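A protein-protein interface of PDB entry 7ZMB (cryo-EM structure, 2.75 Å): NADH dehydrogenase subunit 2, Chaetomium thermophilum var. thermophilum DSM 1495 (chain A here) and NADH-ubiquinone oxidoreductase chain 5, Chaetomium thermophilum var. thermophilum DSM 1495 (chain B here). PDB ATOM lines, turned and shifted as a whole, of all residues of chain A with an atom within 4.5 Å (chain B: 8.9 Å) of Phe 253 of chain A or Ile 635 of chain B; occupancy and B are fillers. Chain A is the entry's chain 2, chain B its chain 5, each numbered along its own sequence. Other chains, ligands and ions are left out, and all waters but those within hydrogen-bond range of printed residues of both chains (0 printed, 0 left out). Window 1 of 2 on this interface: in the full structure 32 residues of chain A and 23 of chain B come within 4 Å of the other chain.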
ATOM      1  N   LEU A 182      30.543  22.108   1.467  1.00  0.00           N
ATOM      2  CA  LEU A 182      29.932  21.388   0.359  1.00  0.00           C
ATOM      3  C   LEU A 182      29.458  22.329  -0.734  1.00  0.00           C
ATOM      4  O   LEU A 182      29.360  21.920  -1.895  1.00  0.00           O
ATOM      5  CB  LEU A 182      28.776  20.536   0.860  1.00  0.00           C
ATOM      6  CG  LEU A 182      29.112  19.281   1.649  1.00  0.00           C
ATOM      7  CD1 LEU A 182      27.827  18.574   1.987  1.00  0.00           C
ATOM      8  CD2 LEU A 182      30.057  18.370   0.890  1.00  0.00           C
ATOM      9  N   GLY A 183      29.147  23.577  -0.389  1.00  0.00           N
ATOM     10  CA  GLY A 183      28.878  24.565  -1.409  1.00  0.00           C
ATOM     11  C   GLY A 183      30.125  25.001  -2.147  1.00  0.00           C
ATOM     12  O   GLY A 183      30.054  25.388  -3.317  1.00  0.00           O
ATOM     13  N   LEU A 185      32.525  22.893  -2.832  1.00  0.00           N
ATOM     14  CA  LEU A 185      32.564  21.832  -3.827  1.00  0.00           C
ATOM     15  C   LEU A 185      31.598  22.124  -4.966  1.00  0.00           C
ATOM     16  O   LEU A 185      31.902  21.861  -6.132  1.00  0.00           O
ATOM     17  CB  LEU A 185      32.235  20.495  -3.174  1.00  0.00           C
ATOM     18  CG  LEU A 185      32.284  19.309  -4.132  1.00  0.00           C
ATOM     19  CD1 LEU A 185      33.661  19.227  -4.742  1.00  0.00           C
ATOM     20  CD2 LEU A 185      31.906  18.014  -3.429  1.00  0.00           C
ATOM     21  N   SER A 186      30.420  22.658  -4.637  1.00  0.00           N
ATOM     22  CA  SER A 186      29.426  22.981  -5.651  1.00  0.00           C
ATOM     23  C   SER A 186      29.932  24.057  -6.600  1.00  0.00           C
ATOM     24  O   SER A 186      29.673  24.008  -7.807  1.00  0.00           O
ATOM     25  CB  SER A 186      28.128  23.419  -4.972  1.00  0.00           C
ATOM     26  OG  SER A 186      27.214  23.986  -5.890  1.00  0.00           O
ATOM     27  N   PHE A 189      32.416  22.927  -9.283  1.00  0.00           N
ATOM     28  CA  PHE A 189      31.747  22.381 -10.459  1.00  0.00           C
ATOM     29  C   PHE A 189      31.244  23.495 -11.365  1.00  0.00           C
ATOM     30  O   PHE A 189      31.319  23.382 -12.589  1.00  0.00           O
ATOM     31  CB  PHE A 189      30.596  21.467 -10.045  1.00  0.00           C
ATOM     32  CG  PHE A 189      31.034  20.139  -9.499  1.00  0.00           C
ATOM     33  CD1 PHE A 189      32.354  19.749  -9.556  1.00  0.00           C
ATOM     34  CD2 PHE A 189      30.120  19.280  -8.912  1.00  0.00           C
ATOM     35  CE1 PHE A 189      32.748  18.525  -9.043  1.00  0.00           C
ATOM     36  CE2 PHE A 189      30.511  18.060  -8.403  1.00  0.00           C
ATOM     37  CZ  PHE A 189      31.820  17.683  -8.471  1.00  0.00           C
ATOM     38  N   ILE A 249      25.071  20.562 -12.428  1.00  0.00           N
ATOM     39  CA  ILE A 249      25.156  19.817 -11.178  1.00  0.00           C
ATOM     40  C   ILE A 249      25.479  20.752 -10.024  1.00  0.00           C
ATOM     41  O   ILE A 249      24.951  20.598  -8.913  1.00  0.00           O
ATOM     42  CB  ILE A 249      26.187  18.678 -11.308  1.00  0.00           C
ATOM     43  CG1 ILE A 249      25.617  17.558 -12.186  1.00  0.00           C
ATOM     44  CG2 ILE A 249      26.650  18.169  -9.936  1.00  0.00           C
ATOM     45  CD1 ILE A 249      26.624  16.517 -12.566  1.00  0.00           C
ATOM     46  N   GLY A 250      26.336  21.744 -10.269  1.00  0.00           N
ATOM     47  CA  GLY A 250      26.653  22.729  -9.258  1.00  0.00           C
ATOM     48  C   GLY A 250      25.466  23.555  -8.818  1.00  0.00           C
ATOM     49  O   GLY A 250      25.478  24.096  -7.714  1.00  0.00           O
ATOM     50  N   PHE A 251      24.438  23.662  -9.653  1.00  0.00           N
ATOM     51  CA  PHE A 251      23.224  24.364  -9.267  1.00  0.00           C
ATOM     52  C   PHE A 251      22.172  23.442  -8.678  1.00  0.00           C
ATOM     53  O   PHE A 251      21.310  23.909  -7.934  1.00  0.00           O
ATOM     54  CB  PHE A 251      22.649  25.118 -10.468  1.00  0.00           C
ATOM     55  CG  PHE A 251      23.394  26.366 -10.794  1.00  0.00           C
ATOM     56  CD1 PHE A 251      23.270  27.485 -10.002  1.00  0.00           C
ATOM     57  CD2 PHE A 251      24.247  26.418 -11.870  1.00  0.00           C
ATOM     58  CE1 PHE A 251      23.973  28.633 -10.294  1.00  0.00           C
ATOM     59  CE2 PHE A 251      24.948  27.567 -12.155  1.00  0.00           C
ATOM     60  CZ  PHE A 251      24.804  28.670 -11.370  1.00  0.00           C
ATOM     61  N   LEU A 252      22.222  22.151  -8.988  1.00  0.00           N
ATOM     62  CA  LEU A 252      21.324  21.205  -8.340  1.00  0.00           C
ATOM     63  C   LEU A 252      21.718  20.964  -6.890  1.00  0.00           C
ATOM     64  O   LEU A 252      20.867  20.596  -6.075  1.00  0.00           O
ATOM     65  CB  LEU A 252      21.289  19.893  -9.119  1.00  0.00           C
ATOM     66  CG  LEU A 252      20.752  20.002 -10.546  1.00  0.00           C
ATOM     67  CD1 LEU A 252      21.054  18.755 -11.337  1.00  0.00           C
ATOM     68  CD2 LEU A 252      19.262  20.291 -10.544  1.00  0.00           C
ATOM     69  N   PHE A 253      22.992  21.165  -6.546  1.00  0.00           N
ATOM     70  CA  PHE A 253      23.374  21.162  -5.141  1.00  0.00           C
ATOM     71  C   PHE A 253      22.702  22.298  -4.392  1.00  0.00           C
ATOM     72  O   PHE A 253      22.177  22.102  -3.292  1.00  0.00           O
ATOM     73  CB  PHE A 253      24.889  21.273  -4.985  1.00  0.00           C
ATOM     74  CG  PHE A 253      25.333  21.417  -3.549  1.00  0.00           C
ATOM     75  CD1 PHE A 253      25.593  20.305  -2.781  1.00  0.00           C
ATOM     76  CD2 PHE A 253      25.457  22.669  -2.961  1.00  0.00           C
ATOM     77  CE1 PHE A 253      25.985  20.442  -1.473  1.00  0.00           C
ATOM     78  CE2 PHE A 253      25.834  22.798  -1.659  1.00  0.00           C
ATOM     79  CZ  PHE A 253      26.098  21.686  -0.914  1.00  0.00           C
ATOM     80  N   LYS A 254      22.705  23.495  -4.978  1.00  0.00           N
ATOM     81  CA  LYS A 254      22.256  24.674  -4.251  1.00  0.00           C
ATOM     82  C   LYS A 254      20.742  24.724  -4.113  1.00  0.00           C
ATOM     83  O   LYS A 254      20.233  25.207  -3.097  1.00  0.00           O
ATOM     84  CB  LYS A 254      22.781  25.926  -4.937  1.00  0.00           C
ATOM     85  CG  LYS A 254      24.283  25.961  -4.999  1.00  0.00           C
ATOM     86  CD  LYS A 254      24.777  26.973  -5.985  1.00  0.00           C
ATOM     87  CE  LYS A 254      26.290  27.049  -5.962  1.00  0.00           C
ATOM     88  NZ  LYS A 254      26.805  27.821  -4.823  1.00  0.00           N
ATOM     89  N   VAL A 255      20.002  24.229  -5.109  1.00  0.00           N
ATOM     90  CA  VAL A 255      18.560  24.092  -4.928  1.00  0.00           C
ATOM     91  C   VAL A 255      18.209  22.847  -4.143  1.00  0.00           C
ATOM     92  O   VAL A 255      17.026  22.618  -3.865  1.00  0.00           O
ATOM     93  CB  VAL A 255      17.805  24.084  -6.270  1.00  0.00           C
ATOM     94  CG1 VAL A 255      17.962  25.430  -6.960  1.00  0.00           C
ATOM     95  CG2 VAL A 255      18.265  22.926  -7.153  1.00  0.00           C
ATOM     96  N   SER A 256      19.207  22.053  -3.758  1.00  0.00           N
ATOM     97  CA  SER A 256      19.017  20.826  -2.995  1.00  0.00           C
ATOM     98  C   SER A 256      18.071  19.866  -3.716  1.00  0.00           C
ATOM     99  O   SER A 256      17.146  19.307  -3.130  1.00  0.00           O
ATOM    100  CB  SER A 256      18.533  21.127  -1.579  1.00  0.00           C
ATOM    101  OG  SER A 256      18.499  19.938  -0.820  1.00  0.00           O
ATOM    102  N   PHE A 260      21.814  15.356  -4.800  1.00  0.00           N
ATOM    103  CA  PHE A 260      22.743  16.302  -4.192  1.00  0.00           C
ATOM    104  C   PHE A 260      22.050  17.083  -3.088  1.00  0.00           C
ATOM    105  O   PHE A 260      22.263  18.283  -2.921  1.00  0.00           O
ATOM    106  CB  PHE A 260      23.314  17.251  -5.238  1.00  0.00           C
ATOM    107  CG  PHE A 260      23.705  16.574  -6.504  1.00  0.00           C
ATOM    108  CD1 PHE A 260      24.910  15.908  -6.602  1.00  0.00           C
ATOM    109  CD2 PHE A 260      22.861  16.594  -7.603  1.00  0.00           C
ATOM    110  CE1 PHE A 260      25.269  15.279  -7.772  1.00  0.00           C
ATOM    111  CE2 PHE A 260      23.215  15.971  -8.770  1.00  0.00           C
ATOM    112  CZ  PHE A 260      24.418  15.310  -8.860  1.00  0.00           C
ATOM    113  N   TRP A 263      22.800  17.679   2.289  1.00  0.00           N
ATOM    114  CA  TRP A 263      23.172  18.749   3.203  1.00  0.00           C
ATOM    115  C   TRP A 263      21.954  19.489   3.745  1.00  0.00           C
ATOM    116  O   TRP A 263      21.926  19.866   4.918  1.00  0.00           O
ATOM    117  CB  TRP A 263      24.114  19.719   2.495  1.00  0.00           C
ATOM    118  CG  TRP A 263      23.467  20.469   1.387  1.00  0.00           C
ATOM    119  CD1 TRP A 263      23.318  20.056   0.104  1.00  0.00           C
ATOM    120  CD2 TRP A 263      22.869  21.765   1.463  1.00  0.00           C
ATOM    121  NE1 TRP A 263      22.669  21.015  -0.632  1.00  0.00           N
ATOM    122  CE2 TRP A 263      22.380  22.074   0.182  1.00  0.00           C
ATOM    123  CE3 TRP A 263      22.693  22.695   2.494  1.00  0.00           C
ATOM    124  CZ2 TRP A 263      21.736  23.270  -0.100  1.00  0.00           C
ATOM    125  CZ3 TRP A 263      22.047  23.877   2.214  1.00  0.00           C
ATOM    126  CH2 TRP A 263      21.577  24.156   0.926  1.00  0.00           C
ATOM    127  N   VAL B 628      30.766  15.532   6.829  1.00  0.00           N
ATOM    128  CA  VAL B 628      30.932  16.301   5.598  1.00  0.00           C
ATOM    129  C   VAL B 628      31.692  15.515   4.538  1.00  0.00           C
ATOM    130  O   VAL B 628      31.402  15.638   3.341  1.00  0.00           O
ATOM    131  CB  VAL B 628      31.611  17.649   5.906  1.00  0.00           C
ATOM    132  CG1 VAL B 628      32.985  17.437   6.534  1.00  0.00           C
ATOM    133  CG2 VAL B 628      31.722  18.491   4.652  1.00  0.00           C
ATOM    134  N   THR B 629      32.589  14.637   4.987  1.00  0.00           N
ATOM    135  CA  THR B 629      33.394  13.859   4.018  1.00  0.00           C
ATOM    136  C   THR B 629      32.483  12.834   3.324  1.00  0.00           C
ATOM    137  O   THR B 629      32.599  12.682   2.094  1.00  0.00           O
ATOM    138  CB  THR B 629      34.756  13.458   4.607  1.00  0.00           C
ATOM    139  OG1 THR B 629      34.623  12.699   5.809  1.00  0.00           O
ATOM    140  CG2 THR B 629      35.641  14.655   4.877  1.00  0.00           C
ATOM    141  N   THR B 630      31.557  12.227   4.069  1.00  0.00           N
ATOM    142  CA  THR B 630      30.632  11.220   3.482  1.00  0.00           C
ATOM    143  C   THR B 630      29.752  11.929   2.470  1.00  0.00           C
ATOM    144  O   THR B 630      29.506  11.368   1.395  1.00  0.00           O
ATOM    145  CB  THR B 630      29.773  10.555   4.565  1.00  0.00           C
ATOM    146  OG1 THR B 630      30.682  10.070   5.550  1.00  0.00           O
ATOM    147  CG2 THR B 630      28.912   9.429   4.040  1.00  0.00           C
ATOM    148  N   TYR B 631      29.316  13.130   2.827  1.00  0.00           N
ATOM    149  CA  TYR B 631      28.414  13.903   1.949  1.00  0.00           C
ATOM    150  C   TYR B 631      29.121  14.279   0.646  1.00  0.00           C
ATOM    151  O   TYR B 631      28.468  14.253  -0.398  1.00  0.00           O
ATOM    152  CB  TYR B 631      27.851  15.085   2.730  1.00  0.00           C
ATOM    153  CG  TYR B 631      26.703  14.737   3.638  1.00  0.00           C
ATOM    154  CD1 TYR B 631      26.257  13.432   3.763  1.00  0.00           C
ATOM    155  CD2 TYR B 631      26.062  15.722   4.361  1.00  0.00           C
ATOM    156  CE1 TYR B 631      25.200  13.112   4.600  1.00  0.00           C
ATOM    157  CE2 TYR B 631      25.004  15.419   5.195  1.00  0.00           C
ATOM    158  CZ  TYR B 631      24.573  14.112   5.312  1.00  0.00           C
ATOM    159  OH  TYR B 631      23.529  13.845   6.144  1.00  0.00           O
ATOM    160  N   ALA B 632      30.399  14.658   0.725  1.00  0.00           N
ATOM    161  CA  ALA B 632      31.174  15.036  -0.481  1.00  0.00           C
ATOM    162  C   ALA B 632      31.287  13.823  -1.390  1.00  0.00           C
ATOM    163  O   ALA B 632      31.162  13.997  -2.607  1.00  0.00           O
ATOM    164  CB  ALA B 632      32.529  15.576  -0.114  1.00  0.00           C
ATOM    165  N   LEU B 633      31.536  12.656  -0.810  1.00  0.00           N
ATOM    166  CA  LEU B 633      31.634  11.405  -1.599  1.00  0.00           C
ATOM    167  C   LEU B 633      30.282  11.126  -2.261  1.00  0.00           C
ATOM    168  O   LEU B 633      30.284  10.771  -3.440  1.00  0.00           O
ATOM    169  CB  LEU B 633      32.084  10.269  -0.681  1.00  0.00           C
ATOM    170  CG  LEU B 633      32.341   8.926  -1.363  1.00  0.00           C
ATOM    171  CD1 LEU B 633      33.126   9.102  -2.653  1.00  0.00           C
ATOM    172  CD2 LEU B 633      33.066   7.984  -0.423  1.00  0.00           C
ATOM    173  N   TYR B 634      29.178  11.361  -1.562  1.00  0.00           N
ATOM    174  CA  TYR B 634      27.850  11.192  -2.202  1.00  0.00           C
ATOM    175  C   TYR B 634      27.734  12.157  -3.393  1.00  0.00           C
ATOM    176  O   TYR B 634      27.257  11.723  -4.461  1.00  0.00           O
ATOM    177  CB  TYR B 634      26.733  11.495  -1.202  1.00  0.00           C
ATOM    178  CG  TYR B 634      26.547  10.574  -0.025  1.00  0.00           C
ATOM    179  CD1 TYR B 634      27.165   9.339   0.057  1.00  0.00           C
ATOM    180  CD2 TYR B 634      25.716  10.950   1.019  1.00  0.00           C
ATOM    181  CE1 TYR B 634      26.971   8.513   1.151  1.00  0.00           C
ATOM    182  CE2 TYR B 634      25.508  10.130   2.113  1.00  0.00           C
ATOM    183  CZ  TYR B 634      26.132   8.901   2.178  1.00  0.00           C
ATOM    184  OH  TYR B 634      25.929   8.102   3.263  1.00  0.00           O
ATOM    185  N   ILE B 635      28.174  13.411  -3.224  1.00  0.00           N
ATOM    186  CA  ILE B 635      28.079  14.431  -4.315  1.00  0.00           C
ATOM    187  C   ILE B 635      28.939  13.997  -5.500  1.00  0.00           C
ATOM    188  O   ILE B 635      28.461  14.134  -6.634  1.00  0.00           O
ATOM    189  CB  ILE B 635      28.421  15.850  -3.833  1.00  0.00           C
ATOM    190  CG1 ILE B 635      27.374  16.367  -2.850  1.00  0.00           C
ATOM    191  CG2 ILE B 635      28.595  16.803  -5.009  1.00  0.00           C
ATOM    192  CD1 ILE B 635      27.828  17.574  -2.078  1.00  0.00           C
ATOM    193  N   LEU B 636      30.149  13.497  -5.231  1.00  0.00           N
ATOM    194  CA  LEU B 636      31.047  13.060  -6.294  1.00  0.00           C
ATOM    195  C   LEU B 636      30.511  11.826  -7.002  1.00  0.00           C
ATOM    196  O   LEU B 636      30.688  11.674  -8.213  1.00  0.00           O
ATOM    197  CB  LEU B 636      32.439  12.796  -5.722  1.00  0.00           C
ATOM    198  CG  LEU B 636      33.534  12.250  -6.638  1.00  0.00           C
ATOM    199  CD1 LEU B 636      33.749  13.164  -7.816  1.00  0.00           C
ATOM    200  CD2 LEU B 636      34.805  12.092  -5.861  1.00  0.00           C
ATOM    201  N   VAL B 637      29.854  10.932  -6.268  1.00  0.00           N
ATOM    202  CA  VAL B 637      29.254   9.757  -6.891  1.00  0.00           C
ATOM    203  C   VAL B 637      28.136  10.164  -7.842  1.00  0.00           C
ATOM    204  O   VAL B 637      28.045   9.657  -8.967  1.00  0.00           O
ATOM    205  CB  VAL B 637      28.760   8.779  -5.813  1.00  0.00           C
ATOM    206  CG1 VAL B 637      27.867   7.718  -6.420  1.00  0.00           C
ATOM    207  CG2 VAL B 637      29.938   8.148  -5.134  1.00  0.00           C
ATOM    208  N   GLY B 638      27.269  11.080  -7.411  1.00  0.00           N
ATOM    209  CA  GLY B 638      26.224  11.559  -8.296  1.00  0.00           C
ATOM    210  C   GLY B 638      26.783  12.331  -9.473  1.00  0.00           C
ATOM    211  O   GLY B 638      26.250  12.264 -10.584  1.00  0.00           O
ATOM    212  N   PHE B 639      27.861  13.078  -9.245  1.00  0.00           N
ATOM    213  CA  PHE B 639      28.560  13.725 -10.343  1.00  0.00           C
ATOM    214  C   PHE B 639      29.089  12.697 -11.332  1.00  0.00           C
ATOM    215  O   PHE B 639      28.989  12.885 -12.546  1.00  0.00           O
ATOM    216  CB  PHE B 639      29.693  14.587  -9.784  1.00  0.00           C
ATOM    217  CG  PHE B 639      30.424  15.390 -10.819  1.00  0.00           C
ATOM    218  CD1 PHE B 639      29.899  16.575 -11.292  1.00  0.00           C
ATOM    219  CD2 PHE B 639      31.646  14.967 -11.303  1.00  0.00           C
ATOM    220  CE1 PHE B 639      30.574  17.324 -12.228  1.00  0.00           C
ATOM    221  CE2 PHE B 639      32.316  15.701 -12.238  1.00  0.00           C
ATOM    222  CZ  PHE B 639      31.779  16.887 -12.699  1.00  0.00           C
ATOM    223  N   ILE B 640      29.640  11.595 -10.832  1.00  0.00           N
ATOM    224  CA  ILE B 640      30.159  10.555 -11.714  1.00  0.00           C
ATOM    225  C   ILE B 640      29.033   9.939 -12.532  1.00  0.00           C
ATOM    226  O   ILE B 640      29.135   9.801 -13.755  1.00  0.00           O
ATOM    227  CB  ILE B 640      30.898   9.482 -10.894  1.00  0.00           C
ATOM    228  CG1 ILE B 640      32.238  10.020 -10.421  1.00  0.00           C
ATOM    229  CG2 ILE B 640      31.103   8.231 -11.723  1.00  0.00           C
ATOM    230  CD1 ILE B 640      33.030  10.593 -11.525  1.00  0.00           C
ATOM    231  N   LEU B 641      27.934   9.571 -11.864  1.00  0.00           N
ATOM    232  CA  LEU B 641      26.864   8.838 -12.524  1.00  0.00           C
ATOM    233  C   LEU B 641      26.146   9.682 -13.568  1.00  0.00           C
ATOM    234  O   LEU B 641      25.672   9.143 -14.570  1.00  0.00           O
ATOM    235  CB  LEU B 641      25.876   8.314 -11.482  1.00  0.00           C
ATOM    236  CG  LEU B 641      26.265   6.979 -10.839  1.00  0.00           C
ATOM    237  CD1 LEU B 641      25.743   6.863  -9.425  1.00  0.00           C
ATOM    238  CD2 LEU B 641      25.771   5.838 -11.691  1.00  0.00           C
ATOM    239  N   TYR B 642      26.046  10.997 -13.355  1.00  0.00           N
ATOM    240  CA  TYR B 642      25.438  11.858 -14.363  1.00  0.00           C
ATOM    241  C   TYR B 642      26.326  11.975 -15.591  1.00  0.00           C
ATOM    242  O   TYR B 642      25.824  12.066 -16.715  1.00  0.00           O
ATOM    243  CB  TYR B 642      25.150  13.246 -13.793  1.00  0.00           C
ATOM    244  CG  TYR B 642      23.856  13.363 -13.030  1.00  0.00           C
ATOM    245  CD1 TYR B 642      23.314  12.279 -12.365  1.00  0.00           C
ATOM    246  CD2 TYR B 642      23.182  14.566 -12.967  1.00  0.00           C
ATOM    247  CE1 TYR B 642      22.132  12.396 -11.661  1.00  0.00           C
ATOM    248  CE2 TYR B 642      22.013  14.692 -12.264  1.00  0.00           C
ATOM    249  CZ  TYR B 642      21.492  13.604 -11.618  1.00  0.00           C
ATOM    250  OH  TYR B 642      20.320  13.727 -10.925  1.00  0.00           O
ATOM    251  N   LEU B 643      27.645  12.023 -15.393  1.00  0.00           N
ATOM    252  CA  LEU B 643      28.562  11.936 -16.522  1.00  0.00           C
ATOM    253  C   LEU B 643      28.433  10.595 -17.229  1.00  0.00           C
ATOM    254  O   LEU B 643      28.345  10.546 -18.459  1.00  0.00           O
ATOM    255  CB  LEU B 643      30.008  12.164 -16.068  1.00  0.00           C
ATOM    256  CG  LEU B 643      30.651  13.556 -15.961  1.00  0.00           C
ATOM    257  CD1 LEU B 643      30.692  14.227 -17.322  1.00  0.00           C
ATOM    258  CD2 LEU B 643      29.954  14.458 -14.976  1.00  0.00           C
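Of the 16 printed residues of chain B, 7 touch a printed residue of chain A.
Printed residues of chain B that touch a printed residue of chain A: Val 628, Tyr 631, Ala 632, Ile 635, Gly 638, Phe 639 and Tyr 642.
Among the printed residues, 13 pairs touch across the chains.
Of chain B, only Ile 635 (3.5 Å) comes within 4 Å of Phe 253 of chain A.
Of the printed residues of chain A, Ile 635 of chain B touches Leu 182 (3.8 Å), Leu 185 (3.9 Å), Phe 253 (3.5 Å) and Phe 260 (3.6 Å).
Printed residues of chain A within 4 Å of Phe 639 of chain B: Phe 189 (3.3 Å), Ile 249 (3.5 Å) and Phe 260 (3.7 Å).
Of the printed residues of chain A, Tyr 642 of chain B touches Ile 249 (3.8 Å) and Phe 260 (3.9 Å).
Leu 643 of chain B touches none of the printed residues of chain A.
The nearest residue of chain B that does not touch Phe 253 of chain A is Tyr 631 of chain B (6.8 Å).
The nearest printed residue of chain A that does not touch Tyr 631 of chain B is Trp 263 of chain A (4.3 Å).
The indole nitrogen (NE1) of Trp 263 of chain A sits at hydrogen-bond distance from the backbone carbonyl oxygen (O) of Phe 253 of chain A, at 2.9 Å.
Leu 182 of chain A touches Val 628 of chain B.
Leu 182 of chain A touches Tyr 631 of chain B.
CD2 of Leu 182 of chain A touches N of Ala 632 of chain B, at 3.7 Å.
Leu 182 of chain A touches Ile 635 of chain B (CD2 to CD1, 3.8 Å).
Phe 189 of chain A touches Phe 639 of chain B (CE2 to CD1, 3.3 Å).
Ile 249 of chain A touches Phe 639 of chain B.
Ile 249 of chain A touches Tyr 642 of chain B (CD1 to CB, 3.8 Å).
CD1 of Ile 635 of chain B touches CE1 of Phe 253 of chain A, at 3.5 Å.
CE1 of Phe 260 of chain A touches O of Ile 635 of chain B, 3.6 Å away.
Phe 260 of chain A touches Phe 639 of chain B (CE1 to N, 3.7 Å).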
